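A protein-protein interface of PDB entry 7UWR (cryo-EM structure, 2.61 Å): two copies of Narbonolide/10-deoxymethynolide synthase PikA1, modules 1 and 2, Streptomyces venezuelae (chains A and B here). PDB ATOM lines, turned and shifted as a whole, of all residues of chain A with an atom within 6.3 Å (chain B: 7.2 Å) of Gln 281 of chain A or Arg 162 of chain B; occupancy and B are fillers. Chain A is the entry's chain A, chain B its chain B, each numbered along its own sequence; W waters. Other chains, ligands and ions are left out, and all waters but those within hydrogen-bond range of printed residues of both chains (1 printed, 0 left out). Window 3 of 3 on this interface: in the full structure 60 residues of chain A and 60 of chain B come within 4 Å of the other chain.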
ATOM      1  N   VAL A 266     -16.284 -11.353 -35.032  1.00  0.00           N
ATOM      2  CA  VAL A 266     -16.591 -12.767 -34.875  1.00  0.00           C
ATOM      3  C   VAL A 266     -15.757 -13.323 -33.728  1.00  0.00           C
ATOM      4  O   VAL A 266     -14.565 -13.021 -33.616  1.00  0.00           O
ATOM      5  CB  VAL A 266     -16.329 -13.559 -36.176  1.00  0.00           C
ATOM      6  CG1 VAL A 266     -16.715 -15.015 -36.003  1.00  0.00           C
ATOM      7  CG2 VAL A 266     -17.098 -12.949 -37.330  1.00  0.00           C
ATOM      8  N   ASN A 267     -16.384 -14.123 -32.869  1.00  0.00           N
ATOM      9  CA  ASN A 267     -15.667 -14.856 -31.832  1.00  0.00           C
ATOM     10  C   ASN A 267     -16.326 -16.224 -31.685  1.00  0.00           C
ATOM     11  O   ASN A 267     -17.343 -16.513 -32.320  1.00  0.00           O
ATOM     12  CB  ASN A 267     -15.565 -14.018 -30.538  1.00  0.00           C
ATOM     13  CG  ASN A 267     -16.686 -14.265 -29.528  1.00  0.00           C
ATOM     14  OD1 ASN A 267     -17.659 -14.975 -29.771  1.00  0.00           O
ATOM     15  ND2 ASN A 267     -16.546 -13.637 -28.370  1.00  0.00           N
ATOM     16  N   ASN A 268     -15.753 -17.078 -30.846  1.00  0.00           N
ATOM     17  CA  ASN A 268     -16.419 -18.310 -30.456  1.00  0.00           C
ATOM     18  C   ASN A 268     -16.780 -18.286 -28.975  1.00  0.00           C
ATOM     19  O   ASN A 268     -16.150 -17.593 -28.175  1.00  0.00           O
ATOM     20  CB  ASN A 268     -15.547 -19.534 -30.770  1.00  0.00           C
ATOM     21  CG  ASN A 268     -16.335 -20.833 -30.732  1.00  0.00           C
ATOM     22  OD1 ASN A 268     -16.526 -21.431 -29.675  1.00  0.00           O
ATOM     23  ND2 ASN A 268     -16.804 -21.270 -31.893  1.00  0.00           N
ATOM     24  N   GLY A 269     -17.831 -19.034 -28.633  1.00  0.00           N
ATOM     25  CA  GLY A 269     -18.178 -19.298 -27.245  1.00  0.00           C
ATOM     26  C   GLY A 269     -17.074 -19.950 -26.442  1.00  0.00           C
ATOM     27  O   GLY A 269     -17.067 -19.838 -25.210  1.00  0.00           O
ATOM     28  N   GLY A 270     -16.136 -20.622 -27.108  1.00  0.00           N
ATOM     29  CA  GLY A 270     -15.096 -21.356 -26.413  1.00  0.00           C
ATOM     30  C   GLY A 270     -15.660 -22.433 -25.511  1.00  0.00           C
ATOM     31  O   GLY A 270     -16.594 -23.156 -25.870  1.00  0.00           O
ATOM     32  N   ALA A 271     -15.094 -22.536 -24.309  1.00  0.00           N
ATOM     33  CA  ALA A 271     -15.510 -23.549 -23.339  1.00  0.00           C
ATOM     34  C   ALA A 271     -16.811 -23.137 -22.647  1.00  0.00           C
ATOM     35  O   ALA A 271     -16.870 -22.886 -21.444  1.00  0.00           O
ATOM     36  CB  ALA A 271     -14.399 -23.796 -22.326  1.00  0.00           C
ATOM     37  N   ASP A 279     -23.085 -18.725 -24.826  1.00  0.00           N
ATOM     38  CA  ASP A 279     -22.320 -18.108 -23.750  1.00  0.00           C
ATOM     39  C   ASP A 279     -22.569 -16.606 -23.779  1.00  0.00           C
ATOM     40  O   ASP A 279     -22.191 -15.924 -24.736  1.00  0.00           O
ATOM     41  CB  ASP A 279     -20.831 -18.431 -23.898  1.00  0.00           C
ATOM     42  CG  ASP A 279     -20.003 -17.950 -22.726  1.00  0.00           C
ATOM     43  OD1 ASP A 279     -20.019 -16.739 -22.423  1.00  0.00           O
ATOM     44  OD2 ASP A 279     -19.332 -18.793 -22.099  1.00  0.00           O
ATOM     45  N   ALA A 280     -23.206 -16.100 -22.721  1.00  0.00           N
ATOM     46  CA  ALA A 280     -23.570 -14.689 -22.659  1.00  0.00           C
ATOM     47  C   ALA A 280     -22.348 -13.785 -22.651  1.00  0.00           C
ATOM     48  O   ALA A 280     -22.387 -12.685 -23.208  1.00  0.00           O
ATOM     49  CB  ALA A 280     -24.436 -14.424 -21.428  1.00  0.00           C
ATOM     50  N   GLN A 281     -21.259 -14.223 -22.022  1.00  0.00           N
ATOM     51  CA  GLN A 281     -20.056 -13.400 -21.944  1.00  0.00           C
ATOM     52  C   GLN A 281     -19.308 -13.347 -23.274  1.00  0.00           C
ATOM     53  O   GLN A 281     -18.792 -12.292 -23.656  1.00  0.00           O
ATOM     54  CB  GLN A 281     -19.147 -13.926 -20.836  1.00  0.00           C
ATOM     55  CG  GLN A 281     -19.859 -14.227 -19.523  1.00  0.00           C
ATOM     56  CD  GLN A 281     -20.942 -13.217 -19.181  1.00  0.00           C
ATOM     57  OE1 GLN A 281     -22.106 -13.575 -19.006  1.00  0.00           O
ATOM     58  NE2 GLN A 281     -20.558 -11.949 -19.069  1.00  0.00           N
ATOM     59  N   ALA A 282     -19.279 -14.452 -24.016  1.00  0.00           N
ATOM     60  CA  ALA A 282     -18.765 -14.416 -25.383  1.00  0.00           C
ATOM     61  C   ALA A 282     -19.637 -13.568 -26.306  1.00  0.00           C
ATOM     62  O   ALA A 282     -19.124 -12.860 -27.179  1.00  0.00           O
ATOM     63  CB  ALA A 282     -18.632 -15.838 -25.926  1.00  0.00           C
ATOM     64  N   GLN A 283     -20.954 -13.600 -26.112  1.00  0.00           N
ATOM     65  CA  GLN A 283     -21.831 -12.724 -26.884  1.00  0.00           C
ATOM     66  C   GLN A 283     -21.604 -11.251 -26.556  1.00  0.00           C
ATOM     67  O   GLN A 283     -21.538 -10.412 -27.463  1.00  0.00           O
ATOM     68  CB  GLN A 283     -23.283 -13.117 -26.650  1.00  0.00           C
ATOM     69  CG  GLN A 283     -23.657 -14.431 -27.293  1.00  0.00           C
ATOM     70  CD  GLN A 283     -25.070 -14.844 -26.978  1.00  0.00           C
ATOM     71  OE1 GLN A 283     -25.860 -14.050 -26.475  1.00  0.00           O
ATOM     72  NE2 GLN A 283     -25.400 -16.092 -27.274  1.00  0.00           N
ATOM     73  N   GLU A 284     -21.477 -10.917 -25.271  1.00  0.00           N
ATOM     74  CA  GLU A 284     -21.028  -9.587 -24.869  1.00  0.00           C
ATOM     75  C   GLU A 284     -19.722  -9.203 -25.547  1.00  0.00           C
ATOM     76  O   GLU A 284     -19.557  -8.068 -26.004  1.00  0.00           O
ATOM     77  CB  GLU A 284     -20.861  -9.529 -23.353  1.00  0.00           C
ATOM     78  CG  GLU A 284     -22.154  -9.473 -22.587  1.00  0.00           C
ATOM     79  CD  GLU A 284     -21.944  -9.506 -21.095  1.00  0.00           C
ATOM     80  OE1 GLU A 284     -21.088  -8.745 -20.601  1.00  0.00           O
ATOM     81  OE2 GLU A 284     -22.636 -10.290 -20.415  1.00  0.00           O
ATOM     82  N   ALA A 285     -18.763 -10.124 -25.569  1.00  0.00           N
ATOM     83  CA  ALA A 285     -17.463  -9.846 -26.168  1.00  0.00           C
ATOM     84  C   ALA A 285     -17.563  -9.537 -27.658  1.00  0.00           C
ATOM     85  O   ALA A 285     -16.920  -8.598 -28.141  1.00  0.00           O
ATOM     86  CB  ALA A 285     -16.522 -11.024 -25.924  1.00  0.00           C
ATOM     87  N   VAL A 286     -18.394 -10.279 -28.397  1.00  0.00           N
ATOM     88  CA  VAL A 286     -18.635  -9.931 -29.800  1.00  0.00           C
ATOM     89  C   VAL A 286     -19.291  -8.569 -29.922  1.00  0.00           C
ATOM     90  O   VAL A 286     -18.901  -7.751 -30.761  1.00  0.00           O
ATOM     91  CB  VAL A 286     -19.510 -10.989 -30.498  1.00  0.00           C
ATOM     92  CG1 VAL A 286     -19.497 -10.772 -31.998  1.00  0.00           C
ATOM     93  CG2 VAL A 286     -19.048 -12.326 -30.192  1.00  0.00           C
ATOM     94  N   ILE A 317     -30.070 -15.686 -22.396  1.00  0.00           N
ATOM     95  CA  ILE A 317     -28.638 -15.427 -22.531  1.00  0.00           C
ATOM     96  C   ILE A 317     -28.365 -14.288 -23.508  1.00  0.00           C
ATOM     97  O   ILE A 317     -27.548 -13.396 -23.234  1.00  0.00           O
ATOM     98  CB  ILE A 317     -27.924 -16.724 -22.957  1.00  0.00           C
ATOM     99  CG1 ILE A 317     -27.742 -17.646 -21.754  1.00  0.00           C
ATOM    100  CG2 ILE A 317     -26.595 -16.429 -23.628  1.00  0.00           C
ATOM    101  CD1 ILE A 317     -27.386 -19.057 -22.131  1.00  0.00           C
ATOM    102  N   ALA A 321     -26.730 -10.656 -22.436  1.00  0.00           N
ATOM    103  CA  ALA A 321     -25.586 -10.070 -23.132  1.00  0.00           C
ATOM    104  C   ALA A 321     -25.905  -8.713 -23.750  1.00  0.00           C
ATOM    105  O   ALA A 321     -25.083  -7.793 -23.688  1.00  0.00           O
ATOM    106  CB  ALA A 321     -25.081 -11.034 -24.202  1.00  0.00           C
ATOM    107  N   ALA A 324     -26.092  -6.153 -20.984  1.00  0.00           N
ATOM    108  CA  ALA A 324     -24.762  -5.900 -20.445  1.00  0.00           C
ATOM    109  C   ALA A 324     -23.871  -5.121 -21.408  1.00  0.00           C
ATOM    110  O   ALA A 324     -22.966  -4.405 -20.965  1.00  0.00           O
ATOM    111  CB  ALA A 324     -24.100  -7.219 -20.061  1.00  0.00           C
ATOM    112  N   LEU B 110      -4.867 -22.210 -22.991  1.00  0.00           N
ATOM    113  CA  LEU B 110      -5.448 -21.323 -23.990  1.00  0.00           C
ATOM    114  C   LEU B 110      -6.912 -20.989 -23.748  1.00  0.00           C
ATOM    115  O   LEU B 110      -7.513 -20.304 -24.582  1.00  0.00           O
ATOM    116  CB  LEU B 110      -5.295 -21.922 -25.384  1.00  0.00           C
ATOM    117  CG  LEU B 110      -3.861 -22.171 -25.822  1.00  0.00           C
ATOM    118  CD1 LEU B 110      -3.865 -22.824 -27.178  1.00  0.00           C
ATOM    119  CD2 LEU B 110      -3.091 -20.864 -25.849  1.00  0.00           C
ATOM    120  N   THR B 111      -7.511 -21.473 -22.663  1.00  0.00           N
ATOM    121  CA  THR B 111      -8.902 -21.146 -22.372  1.00  0.00           C
ATOM    122  C   THR B 111      -9.091 -19.637 -22.272  1.00  0.00           C
ATOM    123  O   THR B 111      -8.314 -18.944 -21.610  1.00  0.00           O
ATOM    124  CB  THR B 111      -9.348 -21.822 -21.074  1.00  0.00           C
ATOM    125  OG1 THR B 111      -9.274 -23.244 -21.221  1.00  0.00           O
ATOM    126  CG2 THR B 111     -10.774 -21.443 -20.740  1.00  0.00           C
ATOM    127  N   GLY B 112     -10.119 -19.127 -22.951  1.00  0.00           N
ATOM    128  CA  GLY B 112     -10.420 -17.711 -22.969  1.00  0.00           C
ATOM    129  C   GLY B 112      -9.564 -16.857 -23.879  1.00  0.00           C
ATOM    130  O   GLY B 112      -9.865 -15.669 -24.042  1.00  0.00           O
ATOM    131  N   THR B 113      -8.509 -17.408 -24.469  1.00  0.00           N
ATOM    132  CA  THR B 113      -7.668 -16.642 -25.378  1.00  0.00           C
ATOM    133  C   THR B 113      -8.366 -16.395 -26.713  1.00  0.00           C
ATOM    134  O   THR B 113      -9.190 -17.189 -27.171  1.00  0.00           O
ATOM    135  CB  THR B 113      -6.336 -17.354 -25.601  1.00  0.00           C
ATOM    136  OG1 THR B 113      -6.553 -18.569 -26.328  1.00  0.00           O
ATOM    137  CG2 THR B 113      -5.681 -17.669 -24.268  1.00  0.00           C
ATOM    138  N   ARG B 114      -8.024 -15.265 -27.331  1.00  0.00           N
ATOM    139  CA  ARG B 114      -8.408 -14.940 -28.701  1.00  0.00           C
ATOM    140  C   ARG B 114      -7.627 -15.778 -29.707  1.00  0.00           C
ATOM    141  O   ARG B 114      -6.866 -15.237 -30.513  1.00  0.00           O
ATOM    142  CB  ARG B 114      -8.197 -13.451 -28.978  1.00  0.00           C
ATOM    143  CG  ARG B 114      -9.131 -12.542 -28.210  1.00  0.00           C
ATOM    144  CD  ARG B 114      -8.661 -11.095 -28.249  1.00  0.00           C
ATOM    145  NE  ARG B 114      -8.688 -10.536 -29.595  1.00  0.00           N
ATOM    146  CZ  ARG B 114      -9.759  -9.996 -30.162  1.00  0.00           C
ATOM    147  NH1 ARG B 114     -10.955 -10.086 -29.606  1.00  0.00           N
ATOM    148  NH2 ARG B 114      -9.635  -9.398 -31.343  1.00  0.00           N
ATOM    149  N   THR B 115      -7.792 -17.096 -29.655  1.00  0.00           N
ATOM    150  CA  THR B 115      -7.164 -18.012 -30.597  1.00  0.00           C
ATOM    151  C   THR B 115      -8.174 -18.457 -31.649  1.00  0.00           C
ATOM    152  O   THR B 115      -9.203 -19.054 -31.316  1.00  0.00           O
ATOM    153  CB  THR B 115      -6.572 -19.222 -29.873  1.00  0.00           C
ATOM    154  OG1 THR B 115      -5.590 -18.778 -28.930  1.00  0.00           O
ATOM    155  CG2 THR B 115      -5.916 -20.166 -30.869  1.00  0.00           C
ATOM    156  N   GLY B 116      -7.875 -18.155 -32.912  1.00  0.00           N
ATOM    157  CA  GLY B 116      -8.752 -18.538 -34.005  1.00  0.00           C
ATOM    158  C   GLY B 116      -8.533 -19.970 -34.461  1.00  0.00           C
ATOM    159  O   GLY B 116      -7.435 -20.515 -34.383  1.00  0.00           O
ATOM    160  N   SER B 156     -12.461 -25.307 -30.893  1.00  0.00           N
ATOM    161  CA  SER B 156     -12.570 -24.087 -30.102  1.00  0.00           C
ATOM    162  C   SER B 156     -13.243 -24.342 -28.760  1.00  0.00           C
ATOM    163  O   SER B 156     -12.819 -23.802 -27.734  1.00  0.00           O
ATOM    164  CB  SER B 156     -13.327 -23.011 -30.877  1.00  0.00           C
ATOM    165  OG  SER B 156     -12.863 -22.931 -32.203  1.00  0.00           O
ATOM    166  N   LEU B 159     -10.705 -26.653 -26.273  1.00  0.00           N
ATOM    167  CA  LEU B 159      -9.602 -25.811 -25.836  1.00  0.00           C
ATOM    168  C   LEU B 159     -10.049 -24.468 -25.276  1.00  0.00           C
ATOM    169  O   LEU B 159      -9.208 -23.715 -24.779  1.00  0.00           O
ATOM    170  CB  LEU B 159      -8.631 -25.605 -26.999  1.00  0.00           C
ATOM    171  CG  LEU B 159      -7.610 -26.705 -27.307  1.00  0.00           C
ATOM    172  CD1 LEU B 159      -8.196 -28.102 -27.312  1.00  0.00           C
ATOM    173  CD2 LEU B 159      -7.054 -26.425 -28.665  1.00  0.00           C
ATOM    174  N   GLY B 160     -11.340 -24.156 -25.332  1.00  0.00           N
ATOM    175  CA  GLY B 160     -11.842 -22.910 -24.794  1.00  0.00           C
ATOM    176  C   GLY B 160     -11.460 -21.679 -25.580  1.00  0.00           C
ATOM    177  O   GLY B 160     -11.435 -20.581 -25.022  1.00  0.00           O
ATOM    178  N   LEU B 161     -11.153 -21.835 -26.865  1.00  0.00           N
ATOM    179  CA  LEU B 161     -10.674 -20.725 -27.677  1.00  0.00           C
ATOM    180  C   LEU B 161     -11.805 -19.737 -27.940  1.00  0.00           C
ATOM    181  O   LEU B 161     -12.890 -20.125 -28.382  1.00  0.00           O
ATOM    182  CB  LEU B 161     -10.079 -21.238 -28.984  1.00  0.00           C
ATOM    183  CG  LEU B 161      -9.142 -22.433 -28.809  1.00  0.00           C
ATOM    184  CD1 LEU B 161      -8.547 -22.841 -30.135  1.00  0.00           C
ATOM    185  CD2 LEU B 161      -8.044 -22.103 -27.808  1.00  0.00           C
ATOM    186  N   ARG B 162     -11.552 -18.460 -27.669  1.00  0.00           N
ATOM    187  CA  ARG B 162     -12.563 -17.431 -27.865  1.00  0.00           C
ATOM    188  C   ARG B 162     -12.474 -16.737 -29.219  1.00  0.00           C
ATOM    189  O   ARG B 162     -13.417 -16.036 -29.592  1.00  0.00           O
ATOM    190  CB  ARG B 162     -12.479 -16.376 -26.753  1.00  0.00           C
ATOM    191  CG  ARG B 162     -13.131 -16.775 -25.436  1.00  0.00           C
ATOM    192  CD  ARG B 162     -14.646 -16.836 -25.602  1.00  0.00           C
ATOM    193  NE  ARG B 162     -15.389 -16.578 -24.373  1.00  0.00           N
ATOM    194  CZ  ARG B 162     -15.636 -15.371 -23.880  1.00  0.00           C
ATOM    195  NH1 ARG B 162     -15.224 -14.275 -24.496  1.00  0.00           N
ATOM    196  NH2 ARG B 162     -16.323 -15.260 -22.748  1.00  0.00           N
ATOM    197  N   GLY B 163     -11.377 -16.905 -29.963  1.00  0.00           N
ATOM    198  CA  GLY B 163     -11.240 -16.268 -31.241  1.00  0.00           C
ATOM    199  C   GLY B 163     -12.220 -16.819 -32.266  1.00  0.00           C
ATOM    200  O   GLY B 163     -12.975 -17.759 -31.998  1.00  0.00           O
ATOM    201  N   PRO B 164     -12.223 -16.215 -33.457  1.00  0.00           N
ATOM    202  CA  PRO B 164     -13.093 -16.700 -34.537  1.00  0.00           C
ATOM    203  C   PRO B 164     -12.873 -18.179 -34.818  1.00  0.00           C
ATOM    204  O   PRO B 164     -11.770 -18.705 -34.665  1.00  0.00           O
ATOM    205  CB  PRO B 164     -12.697 -15.832 -35.737  1.00  0.00           C
ATOM    206  CG  PRO B 164     -12.006 -14.661 -35.164  1.00  0.00           C
ATOM    207  CD  PRO B 164     -11.374 -15.097 -33.890  1.00  0.00           C
ATOM    208  N   SER B 165     -13.936 -18.851 -35.242  1.00  0.00           N
ATOM    209  CA  SER B 165     -13.851 -20.276 -35.532  1.00  0.00           C
ATOM    210  C   SER B 165     -14.798 -20.619 -36.668  1.00  0.00           C
ATOM    211  O   SER B 165     -16.013 -20.456 -36.531  1.00  0.00           O
ATOM    212  CB  SER B 165     -14.182 -21.098 -34.290  1.00  0.00           C
ATOM    213  OG  SER B 165     -14.078 -22.482 -34.545  1.00  0.00           O
ATOM    214  N   GLU B 190      -7.244  -9.525 -34.904  1.00  0.00           N
ATOM    215  CA  GLU B 190      -8.462 -10.204 -34.484  1.00  0.00           C
ATOM    216  C   GLU B 190      -8.136 -11.458 -33.683  1.00  0.00           C
ATOM    217  O   GLU B 190      -8.821 -11.775 -32.706  1.00  0.00           O
ATOM    218  CB  GLU B 190      -9.297 -10.539 -35.721  1.00  0.00           C
ATOM    219  CG  GLU B 190     -10.499 -11.420 -35.492  1.00  0.00           C
ATOM    220  CD  GLU B 190     -11.240 -11.717 -36.784  1.00  0.00           C
ATOM    221  OE1 GLU B 190     -10.694 -12.459 -37.627  1.00  0.00           O
ATOM    222  OE2 GLU B 190     -12.364 -11.203 -36.961  1.00  0.00           O
HETATM  223  O   HOH W   1     -13.747 -10.383 -35.156  1.00  0.00           O
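Water W1 bridges OE2 of Glu 190 of chain B (2.4 Å) and N of Val 266 of chain A (2.7 Å).
Printed residues of chain B that touch a printed residue of chain A: Ser 156, Gly 160, Leu 161, Arg 162, Gly 163, Pro 164 and Ser 165.
Hydrophobic or aromatic side chains of chain B that line the printed part of chain A: Pro 164.
Of the 17 printed residues of chain A, 10 touch a printed residue of chain B.
Printed residues of chain A that touch a printed residue of chain B: Val 266, Asn 267, Asn 268, Gly 269, Gly 270, Ala 271, Asp 279, Gln 281, Ala 282 and Ala 285.
Hydrophobic or aromatic side chains of chain A within 4 Å of the printed part of chain B: Ala 271, Ala 282 and Ala 285.
Among the printed residues, 17 pairs touch across the chains.
Among the printed residues, Asp or Glu carboxylates within 4 Å of a Lys or Arg side-chain nitrogen of the other chain: Asp 279 of chain A with Arg 162 of chain B.
Gln 281 of chain A touches just one residue of chain B: Arg 162.
Of the printed residues of chain B, Ala 285 of chain A touches Arg 162.
Printed residues of chain A within 4 Å of Gly 163 of chain B: Asn 267 and Asn 268.
Of the printed residues of chain B, Gly 269 of chain A touches Arg 162.
Ala 324 of chain A touches none of the printed residues of chain B.
The nearest printed residue of chain B that does not touch Gln 281 of chain A is Gly 112 of chain B (9.6 Å).
The guanidinium group (NH2) of Arg 162 of chain B lies within salt-bridge range of the side-chain carboxylate (OD1) of Asp 279 of chain A (3.99 Å).
N of Asn 268 of chain A lies within hydrogen-bond range of O of Arg 162 of chain B, at 2.8 Å.
NH2 of Arg 162 of chain B lies close to N of Ala 282 of chain A (3.3 Å).
O of Gly 163 of chain B is in hydrogen-bond range of N of Asn 268 of chain A.
Among the printed residues, pairs that only touch across the chains: Val 266 of chain A with Pro 164 of chain B, Asn 267 of chain A with Arg 162 of chain B, Asn 267 of chain A with Gly 163 of chain B, Asn 268 of chain A with Ser 156 of chain B, Asn 268 of chain A with Leu 161 of chain B, Asn 268 of chain A with Ser 165 of chain B, Gly 269 of chain A with Arg 162 of chain B, Gly 270 of chain A with Ser 156 of chain B, Gly 270 of chain A with Gly 160 of chain B, Gly 270 of chain A with Leu 161 of chain B, Ala 271 of chain A with Gly 160 of chain B, Gln 281 of chain A with Arg 162 of chain B and Ala 285 of chain A with Arg 162 of chain B.
No position is printed for both chains.
Of the 17 pairs that touch across the chains among the printed residues, none has its exchanged pair printed and touching as well.
The backbone NH (N) of Gly 163 of chain B lies within hydrogen-bond range of the backbone carbonyl oxygen (O) of Thr 115 of chain B (3.3 Å).
O of Ser 156 of chain B is in hydrogen-bond range of N of Leu 161 of chain B, at 2.7 Å.
The backbone carbonyl oxygen (O) of Thr 113 of chain B lies within hydrogen-bond range of the backbone NH (N) of Arg 162 of chain B (2.7 Å).
The side-chain hydroxyl (OG) of Ser 156 of chain B lies within hydrogen-bond range of the side-chain hydroxyl (OG) of Ser 165 of chain B, at 2.7 Å.
N of Gln 281 of chain A sits at hydrogen-bond distance from OD1 of Asp 279 of chain A.
OD1 of Asp 279 of chain A lies within hydrogen-bond range of N of Ala 282 of chain A.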
